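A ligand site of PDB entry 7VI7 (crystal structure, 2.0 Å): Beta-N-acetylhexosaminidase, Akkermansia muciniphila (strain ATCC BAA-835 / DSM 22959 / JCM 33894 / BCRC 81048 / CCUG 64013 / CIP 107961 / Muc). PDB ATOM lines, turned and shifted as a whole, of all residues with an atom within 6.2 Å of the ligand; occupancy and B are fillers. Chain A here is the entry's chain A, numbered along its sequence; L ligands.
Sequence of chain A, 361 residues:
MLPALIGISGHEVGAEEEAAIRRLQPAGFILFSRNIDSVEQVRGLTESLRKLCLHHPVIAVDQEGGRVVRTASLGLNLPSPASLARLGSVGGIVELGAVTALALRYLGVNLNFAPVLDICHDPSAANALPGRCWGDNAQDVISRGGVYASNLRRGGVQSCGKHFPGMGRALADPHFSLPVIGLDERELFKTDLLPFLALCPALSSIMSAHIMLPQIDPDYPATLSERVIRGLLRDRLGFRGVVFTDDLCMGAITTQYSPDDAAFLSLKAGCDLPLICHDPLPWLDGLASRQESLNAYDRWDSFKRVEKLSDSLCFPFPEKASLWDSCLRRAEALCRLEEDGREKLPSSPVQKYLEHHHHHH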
ATOM      1  N   ILE A  30      11.445 -23.172 -19.586  1.00  0.00           N
ATOM      2  CA  ILE A  30      11.858 -23.742 -18.318  1.00  0.00           C
ATOM      3  C   ILE A  30      11.050 -23.082 -17.214  1.00  0.00           C
ATOM      4  O   ILE A  30      10.937 -21.850 -17.180  1.00  0.00           O
ATOM      5  CB  ILE A  30      13.368 -23.576 -18.080  1.00  0.00           C
ATOM      6  CG1 ILE A  30      13.723 -24.023 -16.660  1.00  0.00           C
ATOM      7  CG2 ILE A  30      13.822 -22.153 -18.358  1.00  0.00           C
ATOM      8  CD1 ILE A  30      15.186 -23.992 -16.396  1.00  0.00           C
ATOM      9  N   PHE A  32      10.081 -22.619 -12.989  1.00  0.00           N
ATOM     10  CA  PHE A  32      10.670 -22.509 -11.662  1.00  0.00           C
ATOM     11  C   PHE A  32       9.531 -22.438 -10.640  1.00  0.00           C
ATOM     12  O   PHE A  32       8.342 -22.446 -11.004  1.00  0.00           O
ATOM     13  CB  PHE A  32      11.576 -21.278 -11.551  1.00  0.00           C
ATOM     14  CG  PHE A  32      12.827 -21.356 -12.380  1.00  0.00           C
ATOM     15  CD1 PHE A  32      13.972 -21.955 -11.890  1.00  0.00           C
ATOM     16  CD2 PHE A  32      12.869 -20.801 -13.662  1.00  0.00           C
ATOM     17  CE1 PHE A  32      15.134 -22.025 -12.648  1.00  0.00           C
ATOM     18  CE2 PHE A  32      14.030 -20.865 -14.427  1.00  0.00           C
ATOM     19  CZ  PHE A  32      15.162 -21.477 -13.920  1.00  0.00           C
ATOM     20  N   ASP A  62      13.680 -28.168 -12.985  1.00  0.00           N
ATOM     21  CA  ASP A  62      14.736 -28.772 -12.171  1.00  0.00           C
ATOM     22  C   ASP A  62      14.081 -29.515 -11.004  1.00  0.00           C
ATOM     23  O   ASP A  62      14.068 -29.038  -9.869  1.00  0.00           O
ATOM     24  CB  ASP A  62      15.704 -27.722 -11.655  1.00  0.00           C
ATOM     25  CG  ASP A  62      16.371 -26.926 -12.757  1.00  0.00           C
ATOM     26  OD1 ASP A  62      17.045 -27.542 -13.611  1.00  0.00           O
ATOM     27  OD2 ASP A  62      16.232 -25.680 -12.762  1.00  0.00           O
ATOM     28  N   GLU A  64      14.872 -32.215  -9.018  1.00  0.00           N
ATOM     29  CA  GLU A  64      15.953 -33.136  -8.653  1.00  0.00           C
ATOM     30  C   GLU A  64      15.656 -33.899  -7.371  1.00  0.00           C
ATOM     31  O   GLU A  64      16.086 -35.048  -7.226  1.00  0.00           O
ATOM     32  CB  GLU A  64      17.277 -32.384  -8.486  1.00  0.00           C
ATOM     33  CG  GLU A  64      17.729 -31.613  -9.734  1.00  0.00           C
ATOM     34  CD  GLU A  64      19.018 -30.842  -9.517  1.00  0.00           C
ATOM     35  OE1 GLU A  64      19.737 -31.125  -8.528  1.00  0.00           O
ATOM     36  OE2 GLU A  64      19.309 -29.936 -10.339  1.00  0.00           O
ATOM     37  N   ARG A  70      10.775 -27.883  -7.267  1.00  0.00           N
ATOM     38  CA  ARG A  70       9.999 -26.725  -7.693  1.00  0.00           C
ATOM     39  C   ARG A  70       8.522 -26.825  -7.325  1.00  0.00           C
ATOM     40  O   ARG A  70       7.737 -25.941  -7.710  1.00  0.00           O
ATOM     41  CB  ARG A  70      10.161 -26.509  -9.203  1.00  0.00           C
ATOM     42  CG  ARG A  70      11.605 -26.454  -9.683  1.00  0.00           C
ATOM     43  CD  ARG A  70      12.472 -25.471  -8.901  1.00  0.00           C
ATOM     44  NE  ARG A  70      13.717 -25.186  -9.614  1.00  0.00           N
ATOM     45  CZ  ARG A  70      14.831 -24.753  -9.040  1.00  0.00           C
ATOM     46  NH1 ARG A  70      14.869 -24.568  -7.732  1.00  0.00           N
ATOM     47  NH2 ARG A  70      15.913 -24.523  -9.765  1.00  0.00           N
ATOM     48  N   PHE A 113      15.427 -31.709 -15.828  1.00  0.00           N
ATOM     49  CA  PHE A 113      16.864 -31.460 -15.880  1.00  0.00           C
ATOM     50  C   PHE A 113      17.540 -32.313 -14.813  1.00  0.00           C
ATOM     51  O   PHE A 113      17.974 -31.846 -13.755  1.00  0.00           O
ATOM     52  CB  PHE A 113      17.164 -29.982 -15.700  1.00  0.00           C
ATOM     53  CG  PHE A 113      16.913 -29.160 -16.933  1.00  0.00           C
ATOM     54  CD1 PHE A 113      17.401 -29.577 -18.165  1.00  0.00           C
ATOM     55  CD2 PHE A 113      16.178 -27.984 -16.871  1.00  0.00           C
ATOM     56  CE1 PHE A 113      17.173 -28.830 -19.305  1.00  0.00           C
ATOM     57  CE2 PHE A 113      15.950 -27.236 -18.010  1.00  0.00           C
ATOM     58  CZ  PHE A 113      16.440 -27.668 -19.228  1.00  0.00           C
ATOM     59  N   VAL A 116      21.638 -35.355 -12.179  1.00  0.00           N
ATOM     60  CA  VAL A 116      22.978 -34.815 -11.969  1.00  0.00           C
ATOM     61  C   VAL A 116      23.975 -35.969 -12.004  1.00  0.00           C
ATOM     62  O   VAL A 116      23.874 -36.924 -11.233  1.00  0.00           O
ATOM     63  CB  VAL A 116      23.044 -34.057 -10.637  1.00  0.00           C
ATOM     64  CG1 VAL A 116      24.475 -33.749 -10.254  1.00  0.00           C
ATOM     65  CG2 VAL A 116      22.198 -32.777 -10.701  1.00  0.00           C
ATOM     66  N   ASP A 118      27.339 -35.243 -11.918  1.00  0.00           N
ATOM     67  CA  ASP A 118      28.540 -34.778 -11.250  1.00  0.00           C
ATOM     68  C   ASP A 118      28.947 -35.765 -10.164  1.00  0.00           C
ATOM     69  O   ASP A 118      28.096 -36.351  -9.484  1.00  0.00           O
ATOM     70  CB  ASP A 118      28.319 -33.403 -10.620  1.00  0.00           C
ATOM     71  CG  ASP A 118      27.895 -32.353 -11.644  1.00  0.00           C
ATOM     72  OD1 ASP A 118      28.318 -32.429 -12.817  1.00  0.00           O
ATOM     73  OD2 ASP A 118      27.137 -31.428 -11.251  1.00  0.00           O
ATOM     74  N   LEU A 129      24.707 -25.882  -2.724  1.00  0.00           N
ATOM     75  CA  LEU A 129      23.523 -26.732  -2.775  1.00  0.00           C
ATOM     76  C   LEU A 129      23.934 -28.175  -2.494  1.00  0.00           C
ATOM     77  O   LEU A 129      24.341 -28.901  -3.418  1.00  0.00           O
ATOM     78  CB  LEU A 129      22.801 -26.619  -4.124  1.00  0.00           C
ATOM     79  CG  LEU A 129      21.752 -25.516  -4.231  1.00  0.00           C
ATOM     80  CD1 LEU A 129      21.111 -25.501  -5.627  1.00  0.00           C
ATOM     81  CD2 LEU A 129      20.687 -25.675  -3.159  1.00  0.00           C
ATOM     82  N   ARG A 132      23.021 -32.947  -4.189  1.00  0.00           N
ATOM     83  CA  ARG A 132      22.620 -33.133  -5.578  1.00  0.00           C
ATOM     84  C   ARG A 132      23.260 -34.335  -6.245  1.00  0.00           C
ATOM     85  O   ARG A 132      22.778 -34.763  -7.303  1.00  0.00           O
ATOM     86  CB  ARG A 132      22.957 -31.888  -6.410  1.00  0.00           C
ATOM     87  CG  ARG A 132      22.265 -30.610  -5.987  1.00  0.00           C
ATOM     88  CD  ARG A 132      22.733 -29.462  -6.869  1.00  0.00           C
ATOM     89  NE  ARG A 132      21.997 -29.412  -8.138  1.00  0.00           N
ATOM     90  CZ  ARG A 132      22.208 -28.488  -9.075  1.00  0.00           C
ATOM     91  NH1 ARG A 132      23.136 -27.561  -8.899  1.00  0.00           N
ATOM     92  NH2 ARG A 132      21.498 -28.497 -10.195  1.00  0.00           N
ATOM     93  N   LYS A 162      23.682 -33.782 -16.477  1.00  0.00           N
ATOM     94  CA  LYS A 162      24.329 -32.510 -16.192  1.00  0.00           C
ATOM     95  C   LYS A 162      25.278 -32.714 -15.021  1.00  0.00           C
ATOM     96  O   LYS A 162      25.067 -33.610 -14.196  1.00  0.00           O
ATOM     97  CB  LYS A 162      23.289 -31.423 -15.881  1.00  0.00           C
ATOM     98  CG  LYS A 162      22.502 -31.635 -14.593  1.00  0.00           C
ATOM     99  CD  LYS A 162      21.337 -30.632 -14.521  1.00  0.00           C
ATOM    100  CE  LYS A 162      20.721 -30.597 -13.132  1.00  0.00           C
ATOM    101  NZ  LYS A 162      19.577 -29.638 -13.049  1.00  0.00           N
ATOM    102  N   HIS A 163      26.341 -31.911 -14.948  1.00  0.00           N
ATOM    103  CA  HIS A 163      26.655 -30.855 -15.920  1.00  0.00           C
ATOM    104  C   HIS A 163      27.953 -31.182 -16.674  1.00  0.00           C
ATOM    105  O   HIS A 163      29.031 -31.193 -16.082  1.00  0.00           O
ATOM    106  CB  HIS A 163      26.788 -29.514 -15.201  1.00  0.00           C
ATOM    107  CG  HIS A 163      25.691 -29.217 -14.228  1.00  0.00           C
ATOM    108  ND1 HIS A 163      25.623 -29.788 -12.975  1.00  0.00           N
ATOM    109  CD2 HIS A 163      24.623 -28.397 -14.315  1.00  0.00           C
ATOM    110  CE1 HIS A 163      24.559 -29.340 -12.333  1.00  0.00           C
ATOM    111  NE2 HIS A 163      23.928 -28.489 -13.128  1.00  0.00           N
ATOM    112  N   MET A 167      31.017 -31.439 -13.184  1.00  0.00           N
ATOM    113  CA  MET A 167      31.270 -30.314 -12.294  1.00  0.00           C
ATOM    114  C   MET A 167      32.022 -30.710 -11.027  1.00  0.00           C
ATOM    115  O   MET A 167      32.534 -29.815 -10.341  1.00  0.00           O
ATOM    116  CB  MET A 167      29.953 -29.650 -11.909  1.00  0.00           C
ATOM    117  CG  MET A 167      29.392 -28.752 -12.985  1.00  0.00           C
ATOM    118  SD  MET A 167      29.710 -27.027 -12.622  1.00  0.00           S
ATOM    119  CE  MET A 167      29.007 -26.906 -10.975  1.00  0.00           C
ATOM    120  N   MET A 207      23.317 -31.242 -20.530  1.00  0.00           N
ATOM    121  CA  MET A 207      23.500 -29.815 -20.304  1.00  0.00           C
ATOM    122  C   MET A 207      24.974 -29.530 -20.060  1.00  0.00           C
ATOM    123  O   MET A 207      25.611 -30.161 -19.206  1.00  0.00           O
ATOM    124  CB  MET A 207      22.668 -29.319 -19.106  1.00  0.00           C
ATOM    125  CG  MET A 207      22.901 -27.863 -18.786  1.00  0.00           C
ATOM    126  SD  MET A 207      22.026 -27.312 -17.307  1.00  0.00           S
ATOM    127  CE  MET A 207      20.322 -27.644 -17.745  1.00  0.00           C
ATOM    128  N   ALA A 209      28.107 -27.068 -18.851  1.00  0.00           N
ATOM    129  CA  ALA A 209      28.344 -26.073 -17.821  1.00  0.00           C
ATOM    130  C   ALA A 209      29.315 -25.000 -18.303  1.00  0.00           C
ATOM    131  O   ALA A 209      30.046 -25.180 -19.283  1.00  0.00           O
ATOM    132  CB  ALA A 209      28.883 -26.736 -16.543  1.00  0.00           C
ATOM    133  N   HIS A 210      29.323 -23.878 -17.576  1.00  0.00           N
ATOM    134  CA  HIS A 210      30.194 -22.735 -17.883  1.00  0.00           C
ATOM    135  C   HIS A 210      31.548 -22.934 -17.191  1.00  0.00           C
ATOM    136  O   HIS A 210      31.926 -22.222 -16.266  1.00  0.00           O
ATOM    137  CB  HIS A 210      29.551 -21.436 -17.430  1.00  0.00           C
ATOM    138  CG  HIS A 210      28.244 -21.127 -18.091  1.00  0.00           C
ATOM    139  ND1 HIS A 210      28.011 -21.332 -19.442  1.00  0.00           N
ATOM    140  CD2 HIS A 210      27.090 -20.614 -17.601  1.00  0.00           C
ATOM    141  CE1 HIS A 210      26.781 -20.967 -19.734  1.00  0.00           C
ATOM    142  NE2 HIS A 210      26.204 -20.523 -18.636  1.00  0.00           N
ATOM    143  N   THR A 245      22.537 -25.503 -22.568  1.00  0.00           N
ATOM    144  CA  THR A 245      23.543 -24.748 -21.824  1.00  0.00           C
ATOM    145  C   THR A 245      23.057 -24.510 -20.404  1.00  0.00           C
ATOM    146  O   THR A 245      21.852 -24.506 -20.126  1.00  0.00           O
ATOM    147  CB  THR A 245      23.831 -23.390 -22.486  1.00  0.00           C
ATOM    148  OG1 THR A 245      22.722 -22.500 -22.235  1.00  0.00           O
ATOM    149  CG2 THR A 245      24.046 -23.548 -23.986  1.00  0.00           C
ATOM    150  N   ASP A 246      24.025 -24.307 -19.509  1.00  0.00           N
ATOM    151  CA  ASP A 246      23.757 -23.707 -18.203  1.00  0.00           C
ATOM    152  C   ASP A 246      23.031 -22.376 -18.397  1.00  0.00           C
ATOM    153  O   ASP A 246      23.109 -21.782 -19.489  1.00  0.00           O
ATOM    154  CB  ASP A 246      25.064 -23.497 -17.444  1.00  0.00           C
ATOM    155  CG  ASP A 246      25.178 -24.367 -16.204  1.00  0.00           C
ATOM    156  OD1 ASP A 246      24.208 -25.105 -15.899  1.00  0.00           O
ATOM    157  OD2 ASP A 246      26.228 -24.313 -15.531  1.00  0.00           O
ATOM    158  N   ASP A 247      22.339 -21.896 -17.366  1.00  0.00           N
ATOM    159  CA  ASP A 247      21.605 -20.641 -17.478  1.00  0.00           C
ATOM    160  C   ASP A 247      22.544 -19.514 -17.905  1.00  0.00           C
ATOM    161  O   ASP A 247      23.656 -19.378 -17.382  1.00  0.00           O
ATOM    162  CB  ASP A 247      20.943 -20.266 -16.147  1.00  0.00           C
ATOM    163  CG  ASP A 247      20.221 -18.927 -16.206  1.00  0.00           C
ATOM    164  OD1 ASP A 247      19.747 -18.538 -17.282  1.00  0.00           O
ATOM    165  OD2 ASP A 247      20.135 -18.249 -15.162  1.00  0.00           O
ATOM    166  N   LEU A 248      22.089 -18.707 -18.855  1.00  0.00           N
ATOM    167  CA  LEU A 248      22.887 -17.599 -19.358  1.00  0.00           C
ATOM    168  C   LEU A 248      22.587 -16.275 -18.659  1.00  0.00           C
ATOM    169  O   LEU A 248      23.260 -15.284 -18.942  1.00  0.00           O
ATOM    170  CB  LEU A 248      22.673 -17.448 -20.869  1.00  0.00           C
ATOM    171  CG  LEU A 248      23.039 -18.677 -21.691  1.00  0.00           C
ATOM    172  CD1 LEU A 248      22.784 -18.464 -23.166  1.00  0.00           C
ATOM    173  CD2 LEU A 248      24.498 -19.022 -21.457  1.00  0.00           C
ATOM    174  N   LEU A 275      19.900 -21.820 -22.527  1.00  0.00           N
ATOM    175  CA  LEU A 275      18.893 -21.535 -21.518  1.00  0.00           C
ATOM    176  C   LEU A 275      18.930 -20.061 -21.178  1.00  0.00           C
ATOM    177  O   LEU A 275      19.940 -19.560 -20.654  1.00  0.00           O
ATOM    178  CB  LEU A 275      19.102 -22.386 -20.267  1.00  0.00           C
ATOM    179  CG  LEU A 275      18.247 -23.649 -20.106  1.00  0.00           C
ATOM    180  CD1 LEU A 275      18.422 -24.583 -21.282  1.00  0.00           C
ATOM    181  CD2 LEU A 275      18.580 -24.354 -18.794  1.00  0.00           C
ATOM    182  N   CYS A 277      16.924 -18.094 -18.795  1.00  0.00           N
ATOM    183  CA  CYS A 277      15.961 -18.476 -17.768  1.00  0.00           C
ATOM    184  C   CYS A 277      15.237 -17.298 -17.131  1.00  0.00           C
ATOM    185  O   CYS A 277      14.058 -17.425 -16.773  1.00  0.00           O
ATOM    186  CB  CYS A 277      16.669 -19.268 -16.657  1.00  0.00           C
ATOM    187  SG  CYS A 277      17.316 -20.893 -17.163  1.00  0.00           S
ATOM    188  N   HIS A 278      15.908 -16.167 -16.930  1.00  0.00           N
ATOM    189  CA  HIS A 278      15.377 -15.083 -16.108  1.00  0.00           C
ATOM    190  C   HIS A 278      15.422 -13.789 -16.894  1.00  0.00           C
ATOM    191  O   HIS A 278      16.491 -13.359 -17.340  1.00  0.00           O
ATOM    192  CB  HIS A 278      16.162 -14.973 -14.799  1.00  0.00           C
ATOM    193  CG  HIS A 278      16.340 -16.278 -14.099  1.00  0.00           C
ATOM    194  ND1 HIS A 278      15.294 -16.972 -13.536  1.00  0.00           N
ATOM    195  CD2 HIS A 278      17.443 -17.043 -13.892  1.00  0.00           C
ATOM    196  CE1 HIS A 278      15.737 -18.097 -13.005  1.00  0.00           C
ATOM    197  NE2 HIS A 278      17.044 -18.157 -13.193  1.00  0.00           N
HETATM  198  C1  LIG L   1      21.720 -23.605 -13.955  1.00  0.00           C
HETATM  199  C2  LIG L   1      22.076 -24.872 -13.123  1.00  0.00           C
HETATM  200  C3  LIG L   1      21.386 -26.139 -13.664  1.00  0.00           C
HETATM  201  C4  LIG L   1      19.920 -25.879 -13.911  1.00  0.00           C
HETATM  202  C5  LIG L   1      19.767 -24.675 -14.851  1.00  0.00           C
HETATM  203  C6  LIG L   1      18.306 -24.336 -15.049  1.00  0.00           C
HETATM  204  C7  LIG L   1      24.104 -25.471 -11.858  1.00  0.00           C
HETATM  205  C8  LIG L   1      25.607 -25.724 -11.957  1.00  0.00           C
HETATM  206  O1  LIG L   1      20.315 -23.524 -14.213  1.00  0.00           O
HETATM  207  O2  LIG L   1      21.520 -27.190 -12.714  1.00  0.00           O
HETATM  208  O3  LIG L   1      19.376 -27.068 -14.460  1.00  0.00           O
HETATM  209  O4  LIG L   1      17.709 -23.959 -13.805  1.00  0.00           O
HETATM  210  O5  LIG L   1      23.476 -25.574 -10.798  1.00  0.00           O
HETATM  211  N1  LIG L   1      23.497 -25.140 -13.034  1.00  0.00           N
HETATM  212  O6  LIG L   1      22.452 -23.582 -15.158  1.00  0.00           O
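A ring nitrogen (NE2) of His 210 lies close to the backbone carbonyl oxygen (O) of Asp 246.
The side-chain carboxylate of Asp 62 is in salt-bridge range of the side-chain amino group of Lys 162 (3.3 Å).
The side-chain carboxylate (OD2) of Asp 118 is in hydrogen-bond range of a ring nitrogen (ND1) of His 163, at 2.8 Å.
OE2 of Glu 64 lies within salt-bridge range of NH2 of Arg 132.
The backbone carbonyl oxygen (O) of Asp 247 is in hydrogen-bond range of a ring nitrogen (NE2) of His 210 (3.1 Å).
N of Met 167 sits at hydrogen-bond distance from OD1 of Asp 118 (2.9 Å).
OG1 of Thr 245 is in hydrogen-bond range of N of Leu 275 (2.9 Å).
The backbone carbonyl oxygen (O) of Leu 275 lies within hydrogen-bond range of the backbone NH (N) of Leu 248 (2.9 Å).
CD1 of Ile 30 touches C6 of the ligand, at 3.4 Å.
Phe 32 touches the ligand.
Phe 113 touches the ligand.
CE of Met 167 touches C8 of the ligand, 3.7 Å away.
Met 207 touches the ligand.
Leu 275 touches the ligand.
Hydrophobic or aromatic side chains that line the ligand: Ile 30, Phe 32, Phe 113, His 163, Met 167, Met 207 and Leu 275.
Of the 23 residues printed, 12 come within 4 Å of the ligand.
O6 of the ligand sits at hydrogen-bond distance from OD1 of Asp 246 (2.4 Å).
The side-chain carboxylate (OD2) of Asp 62 lies within hydrogen-bond range of an oxygen (O4) of the ligand (2.5 Å).
NE2 of His 163 lies within hydrogen-bond range of O2 of the ligand, 2.8 Å away.
The guanidinium group (NH1) of Arg 132 is in hydrogen-bond range of an oxygen (O5) of the ligand (2.8 Å).
N of Asp 247 is in hydrogen-bond range of O6 of the ligand, 2.8 Å away.
NZ of Lys 162 lies within hydrogen-bond range of O3 of the ligand (2.9 Å).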
